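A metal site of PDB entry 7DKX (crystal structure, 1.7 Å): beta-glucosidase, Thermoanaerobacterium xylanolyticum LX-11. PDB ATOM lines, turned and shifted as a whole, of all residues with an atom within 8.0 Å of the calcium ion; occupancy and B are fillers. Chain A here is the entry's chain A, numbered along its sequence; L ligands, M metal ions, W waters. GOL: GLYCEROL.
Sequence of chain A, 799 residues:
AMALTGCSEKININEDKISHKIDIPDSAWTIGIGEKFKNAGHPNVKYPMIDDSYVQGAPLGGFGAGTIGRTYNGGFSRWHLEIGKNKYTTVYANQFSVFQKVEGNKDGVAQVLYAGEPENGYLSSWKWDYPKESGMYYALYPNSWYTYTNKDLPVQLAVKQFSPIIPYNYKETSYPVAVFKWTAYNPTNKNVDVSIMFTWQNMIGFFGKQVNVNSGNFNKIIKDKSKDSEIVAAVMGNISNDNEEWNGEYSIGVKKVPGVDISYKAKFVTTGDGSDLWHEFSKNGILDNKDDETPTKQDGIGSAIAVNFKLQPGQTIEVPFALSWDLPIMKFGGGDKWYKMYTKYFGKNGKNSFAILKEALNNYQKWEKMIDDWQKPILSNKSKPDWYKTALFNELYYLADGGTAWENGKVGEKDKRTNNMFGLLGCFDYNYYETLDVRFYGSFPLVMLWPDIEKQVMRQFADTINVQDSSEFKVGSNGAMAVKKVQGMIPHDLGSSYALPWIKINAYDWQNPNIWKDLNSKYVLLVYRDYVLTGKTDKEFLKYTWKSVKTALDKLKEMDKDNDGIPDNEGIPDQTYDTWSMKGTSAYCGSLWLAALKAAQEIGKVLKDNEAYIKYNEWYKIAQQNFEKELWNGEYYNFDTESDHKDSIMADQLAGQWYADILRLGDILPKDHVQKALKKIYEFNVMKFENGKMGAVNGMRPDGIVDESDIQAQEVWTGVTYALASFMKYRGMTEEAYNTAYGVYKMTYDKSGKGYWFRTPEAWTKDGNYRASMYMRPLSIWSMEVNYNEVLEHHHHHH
OD1 of Asp 568 sits close to N of Lys 561, at 2.9 Å.
The backbone NH of Asp 568 is in hydrogen-bond range of the backbone carbonyl oxygen of Met 559.
OG1 of Thr 585 sits at hydrogen-bond distance from OD2 of Asp 564 (3.0 Å).
OD2 of Asp 564 lies close to OE2 of Glu 630 (2.7 Å).
ND2 of Asn 626 lies within hydrogen-bond range of O of Asp 564 (2.8 Å).
The side-chain carboxylate (OD1) of Asp 560 lies close to the backbone NH (N) of Asn 563 (3.1 Å).
OD2 of Asp 560 sits at hydrogen-bond distance from N of Gly 565.
Water W1 lies within hydrogen-bond range of OG1 of Thr 585 (2.7 Å) and O of Pro 567 (2.9 Å).
The calcium ion is bound by the side-chain carboxylate (OD1) of Asp 568 (2.3 Å), the backbone carbonyl oxygen (O) of Ile 566 (2.3 Å), the side-chain carboxylate (OD1) of Asp 564 (2.3 Å), the side-chain carboxylate (OD1) of Asp 560 (2.4 Å), the side-chain carboxylate (OD1) of Asp 562 (2.5 Å) and water W1 (2.5 Å).
Slightly farther from the calcium ion lies O3 of the ligand (3.0 Å).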
ATOM      1  N   LYS A 557      21.544   4.322  -5.072  1.00  0.00           N
ATOM      2  CA  LYS A 557      20.110   4.481  -4.779  1.00  0.00           C
ATOM      3  C   LYS A 557      19.874   5.106  -3.397  1.00  0.00           C
ATOM      4  O   LYS A 557      18.928   5.886  -3.240  1.00  0.00           O
ATOM      5  CB  LYS A 557      19.393   3.124  -4.871  1.00  0.00           C
ATOM      6  CG  LYS A 557      17.875   3.136  -4.693  1.00  0.00           C
ATOM      7  CD  LYS A 557      17.182   4.099  -5.654  1.00  0.00           C
ATOM      8  CE  LYS A 557      15.780   3.644  -6.017  1.00  0.00           C
ATOM      9  NZ  LYS A 557      14.926   3.501  -4.827  1.00  0.00           N
ATOM     10  N   MET A 559      21.429   7.495  -2.093  1.00  0.00           N
ATOM     11  CA  MET A 559      21.607   8.939  -2.205  1.00  0.00           C
ATOM     12  C   MET A 559      20.393   9.675  -2.783  1.00  0.00           C
ATOM     13  O   MET A 559      20.418  10.889  -2.960  1.00  0.00           O
ATOM     14  CB  MET A 559      22.860   9.246  -3.015  1.00  0.00           C
ATOM     15  CG  MET A 559      24.116   8.816  -2.299  1.00  0.00           C
ATOM     16  SD  MET A 559      25.532   8.804  -3.410  1.00  0.00           S
ATOM     17  CE  MET A 559      26.755   8.194  -2.262  1.00  0.00           C
ATOM     18  N   ASP A 560      19.306   8.948  -3.054  1.00  0.00           N
ATOM     19  CA  ASP A 560      18.039   9.576  -3.394  1.00  0.00           C
ATOM     20  C   ASP A 560      17.417  10.118  -2.100  1.00  0.00           C
ATOM     21  O   ASP A 560      16.931   9.347  -1.295  1.00  0.00           O
ATOM     22  CB  ASP A 560      17.130   8.541  -4.058  1.00  0.00           C
ATOM     23  CG  ASP A 560      15.744   9.085  -4.395  1.00  0.00           C
ATOM     24  OD1 ASP A 560      15.536  10.309  -4.432  1.00  0.00           O
ATOM     25  OD2 ASP A 560      14.853   8.256  -4.648  1.00  0.00           O
ATOM     26  N   LYS A 561      17.451  11.431  -1.923  1.00  0.00           N
ATOM     27  CA  LYS A 561      16.936  12.084  -0.710  1.00  0.00           C
ATOM     28  C   LYS A 561      15.411  12.242  -0.669  1.00  0.00           C
ATOM     29  O   LYS A 561      14.821  12.272   0.416  1.00  0.00           O
ATOM     30  CB  LYS A 561      17.551  13.474  -0.546  1.00  0.00           C
ATOM     31  CG  LYS A 561      19.017  13.464  -0.139  1.00  0.00           C
ATOM     32  CD  LYS A 561      19.585  14.862  -0.264  1.00  0.00           C
ATOM     33  CE  LYS A 561      20.982  14.976   0.335  1.00  0.00           C
ATOM     34  NZ  LYS A 561      21.501  16.366   0.183  1.00  0.00           N
ATOM     35  N   ASP A 562      14.771  12.385  -1.826  1.00  0.00           N
ATOM     36  CA  ASP A 562      13.352  12.785  -1.877  1.00  0.00           C
ATOM     37  C   ASP A 562      12.453  11.728  -2.506  1.00  0.00           C
ATOM     38  O   ASP A 562      11.322  12.023  -2.886  1.00  0.00           O
ATOM     39  CB  ASP A 562      13.207  14.105  -2.611  1.00  0.00           C
ATOM     40  CG  ASP A 562      13.590  14.009  -4.072  1.00  0.00           C
ATOM     41  OD1 ASP A 562      14.288  13.035  -4.445  1.00  0.00           O
ATOM     42  OD2 ASP A 562      13.204  14.901  -4.841  1.00  0.00           O
ATOM     43  N   ASN A 563      12.962  10.508  -2.633  1.00  0.00           N
ATOM     44  CA  ASN A 563      12.209   9.376  -3.162  1.00  0.00           C
ATOM     45  C   ASN A 563      11.581   9.621  -4.553  1.00  0.00           C
ATOM     46  O   ASN A 563      10.477   9.176  -4.823  1.00  0.00           O
ATOM     47  CB  ASN A 563      11.148   8.918  -2.136  1.00  0.00           C
ATOM     48  CG  ASN A 563      10.652   7.491  -2.401  1.00  0.00           C
ATOM     49  OD1 ASN A 563      11.375   6.652  -2.937  1.00  0.00           O
ATOM     50  ND2 ASN A 563       9.400   7.235  -2.043  1.00  0.00           N
ATOM     51  N   ASP A 564      12.302  10.322  -5.438  1.00  0.00           N
ATOM     52  CA  ASP A 564      11.901  10.380  -6.856  1.00  0.00           C
ATOM     53  C   ASP A 564      12.573   9.262  -7.686  1.00  0.00           C
ATOM     54  O   ASP A 564      12.390   9.207  -8.900  1.00  0.00           O
ATOM     55  CB  ASP A 564      12.160  11.778  -7.444  1.00  0.00           C
ATOM     56  CG  ASP A 564      13.632  12.043  -7.777  1.00  0.00           C
ATOM     57  OD1 ASP A 564      14.500  11.307  -7.282  1.00  0.00           O
ATOM     58  OD2 ASP A 564      13.915  13.002  -8.509  1.00  0.00           O
ATOM     59  N   GLY A 565      13.323   8.373  -7.017  1.00  0.00           N
ATOM     60  CA  GLY A 565      13.978   7.228  -7.660  1.00  0.00           C
ATOM     61  C   GLY A 565      15.357   7.534  -8.265  1.00  0.00           C
ATOM     62  O   GLY A 565      15.941   6.661  -8.909  1.00  0.00           O
ATOM     63  N   ILE A 566      15.867   8.737  -8.030  1.00  0.00           N
ATOM     64  CA  ILE A 566      17.119   9.226  -8.671  1.00  0.00           C
ATOM     65  C   ILE A 566      18.041   9.803  -7.587  1.00  0.00           C
ATOM     66  O   ILE A 566      17.595  10.601  -6.741  1.00  0.00           O
ATOM     67  CB  ILE A 566      16.809  10.321  -9.718  1.00  0.00           C
ATOM     68  CG1 ILE A 566      15.763   9.841 -10.739  1.00  0.00           C
ATOM     69  CG2 ILE A 566      18.091  10.753 -10.442  1.00  0.00           C
ATOM     70  CD1 ILE A 566      15.155  10.949 -11.575  1.00  0.00           C
ATOM     71  N   PRO A 567      19.339   9.449  -7.598  1.00  0.00           N
ATOM     72  CA  PRO A 567      20.227  10.113  -6.644  1.00  0.00           C
ATOM     73  C   PRO A 567      20.211  11.648  -6.745  1.00  0.00           C
ATOM     74  O   PRO A 567      20.024  12.216  -7.820  1.00  0.00           O
ATOM     75  CB  PRO A 567      21.605   9.528  -6.968  1.00  0.00           C
ATOM     76  CG  PRO A 567      21.496   8.988  -8.357  1.00  0.00           C
ATOM     77  CD  PRO A 567      20.084   8.537  -8.494  1.00  0.00           C
ATOM     78  N   ASP A 568      20.367  12.309  -5.598  1.00  0.00           N
ATOM     79  CA  ASP A 568      20.319  13.766  -5.540  1.00  0.00           C
ATOM     80  C   ASP A 568      21.726  14.344  -5.523  1.00  0.00           C
ATOM     81  O   ASP A 568      22.495  14.049  -4.600  1.00  0.00           O
ATOM     82  CB  ASP A 568      19.621  14.225  -4.259  1.00  0.00           C
ATOM     83  CG  ASP A 568      18.109  14.107  -4.348  1.00  0.00           C
ATOM     84  OD1 ASP A 568      17.599  12.964  -4.336  1.00  0.00           O
ATOM     85  OD2 ASP A 568      17.449  15.152  -4.471  1.00  0.00           O
ATOM     86  N   ASN A 569      22.059  15.191  -6.492  1.00  0.00           N
ATOM     87  CA  ASN A 569      23.285  15.979  -6.405  1.00  0.00           C
ATOM     88  C   ASN A 569      23.122  16.939  -5.232  1.00  0.00           C
ATOM     89  O   ASN A 569      22.023  17.419  -4.970  1.00  0.00           O
ATOM     90  CB  ASN A 569      23.559  16.722  -7.709  1.00  0.00           C
ATOM     91  CG  ASN A 569      23.895  15.775  -8.859  1.00  0.00           C
ATOM     92  OD1 ASN A 569      23.036  15.446  -9.673  1.00  0.00           O
ATOM     93  ND2 ASN A 569      25.144  15.348  -8.936  1.00  0.00           N
ATOM     94  N   GLY A 584      20.012  18.508  -6.810  1.00  0.00           N
ATOM     95  CA  GLY A 584      18.769  17.829  -7.094  1.00  0.00           C
ATOM     96  C   GLY A 584      18.958  16.781  -8.168  1.00  0.00           C
ATOM     97  O   GLY A 584      19.947  16.041  -8.131  1.00  0.00           O
ATOM     98  N   THR A 585      18.035  16.704  -9.124  1.00  0.00           N
ATOM     99  CA  THR A 585      18.170  15.765 -10.236  1.00  0.00           C
ATOM    100  C   THR A 585      18.891  16.538 -11.323  1.00  0.00           C
ATOM    101  O   THR A 585      18.408  17.580 -11.739  1.00  0.00           O
ATOM    102  CB  THR A 585      16.809  15.253 -10.730  1.00  0.00           C
ATOM    103  OG1 THR A 585      16.220  14.411  -9.713  1.00  0.00           O
ATOM    104  CG2 THR A 585      16.944  14.405 -12.007  1.00  0.00           C
ATOM    105  N   TRP A 593      22.457   7.477 -14.559  1.00  0.00           N
ATOM    106  CA  TRP A 593      21.734   6.556 -13.675  1.00  0.00           C
ATOM    107  C   TRP A 593      20.715   5.728 -14.442  1.00  0.00           C
ATOM    108  O   TRP A 593      20.667   4.513 -14.312  1.00  0.00           O
ATOM    109  CB  TRP A 593      21.069   7.385 -12.556  1.00  0.00           C
ATOM    110  CG  TRP A 593      20.121   6.678 -11.627  1.00  0.00           C
ATOM    111  CD1 TRP A 593      18.787   6.949 -11.479  1.00  0.00           C
ATOM    112  CD2 TRP A 593      20.432   5.646 -10.675  1.00  0.00           C
ATOM    113  NE1 TRP A 593      18.256   6.149 -10.507  1.00  0.00           N
ATOM    114  CE2 TRP A 593      19.235   5.331 -10.012  1.00  0.00           C
ATOM    115  CE3 TRP A 593      21.586   4.936 -10.355  1.00  0.00           C
ATOM    116  CZ2 TRP A 593      19.167   4.339  -9.020  1.00  0.00           C
ATOM    117  CZ3 TRP A 593      21.526   3.948  -9.365  1.00  0.00           C
ATOM    118  CH2 TRP A 593      20.309   3.672  -8.705  1.00  0.00           C
ATOM    119  N   ASN A 626      10.202  10.137 -13.753  1.00  0.00           N
ATOM    120  CA  ASN A 626      10.471  11.347 -12.988  1.00  0.00           C
ATOM    121  C   ASN A 626      11.556  12.237 -13.615  1.00  0.00           C
ATOM    122  O   ASN A 626      11.470  13.453 -13.514  1.00  0.00           O
ATOM    123  CB  ASN A 626      10.814  11.010 -11.540  1.00  0.00           C
ATOM    124  CG  ASN A 626       9.599  10.517 -10.770  1.00  0.00           C
ATOM    125  OD1 ASN A 626       8.472  10.880 -11.090  1.00  0.00           O
ATOM    126  ND2 ASN A 626       9.819   9.698  -9.750  1.00  0.00           N
ATOM    127  N   GLU A 630      10.700  16.051 -14.482  1.00  0.00           N
ATOM    128  CA  GLU A 630      11.477  17.089 -13.786  1.00  0.00           C
ATOM    129  C   GLU A 630      12.282  17.995 -14.696  1.00  0.00           C
ATOM    130  O   GLU A 630      12.460  19.170 -14.379  1.00  0.00           O
ATOM    131  CB  GLU A 630      12.418  16.442 -12.767  1.00  0.00           C
ATOM    132  CG  GLU A 630      11.701  15.854 -11.568  1.00  0.00           C
ATOM    133  CD  GLU A 630      12.565  14.894 -10.785  1.00  0.00           C
ATOM    134  OE1 GLU A 630      13.802  14.903 -10.978  1.00  0.00           O
ATOM    135  OE2 GLU A 630      12.004  14.108  -9.987  1.00  0.00           O
ATOM    136  N   THR A 641      17.487  20.433 -11.242  1.00  0.00           N
ATOM    137  CA  THR A 641      16.197  20.892 -10.698  1.00  0.00           C
ATOM    138  C   THR A 641      16.291  21.989  -9.637  1.00  0.00           C
ATOM    139  O   THR A 641      15.275  22.623  -9.334  1.00  0.00           O
ATOM    140  CB  THR A 641      15.412  19.723 -10.084  1.00  0.00           C
ATOM    141  OG1 THR A 641      16.224  19.092  -9.086  1.00  0.00           O
ATOM    142  CG2 THR A 641      15.008  18.727 -11.161  1.00  0.00           C
ATOM    143  N   GLU A 642      17.468  22.214  -9.043  1.00  0.00           N
ATOM    144  CA  GLU A 642      17.597  23.136  -7.886  1.00  0.00           C
ATOM    145  C   GLU A 642      18.677  24.231  -7.928  1.00  0.00           C
ATOM    146  O   GLU A 642      18.686  25.089  -7.038  1.00  0.00           O
ATOM    147  CB  GLU A 642      17.739  22.314  -6.602  1.00  0.00           C
ATOM    148  CG  GLU A 642      16.542  21.418  -6.319  1.00  0.00           C
ATOM    149  CD  GLU A 642      16.687  20.640  -5.026  1.00  0.00           C
ATOM    150  OE1 GLU A 642      17.241  21.197  -4.054  1.00  0.00           O
ATOM    151  OE2 GLU A 642      16.245  19.481  -4.967  1.00  0.00           O
HETATM  152  C1  GOL L   1      13.407  16.698  -8.006  1.00  0.00           C
HETATM  153  O1  GOL L   1      12.290  17.593  -8.095  1.00  0.00           O
HETATM  154  C2  GOL L   1      14.326  17.132  -6.858  1.00  0.00           C
HETATM  155  O2  GOL L   1      14.777  18.483  -7.037  1.00  0.00           O
HETATM  156  C3  GOL L   1      15.568  16.251  -6.793  1.00  0.00           C
HETATM  157  O3  GOL L   1      15.328  14.957  -6.241  1.00  0.00           O
HETATM  158 CA    CA M   1      16.123  12.128  -5.830  1.00  0.00          CA
HETATM  159  O   HOH W   1      17.377  13.429  -7.538  1.00  0.00           O
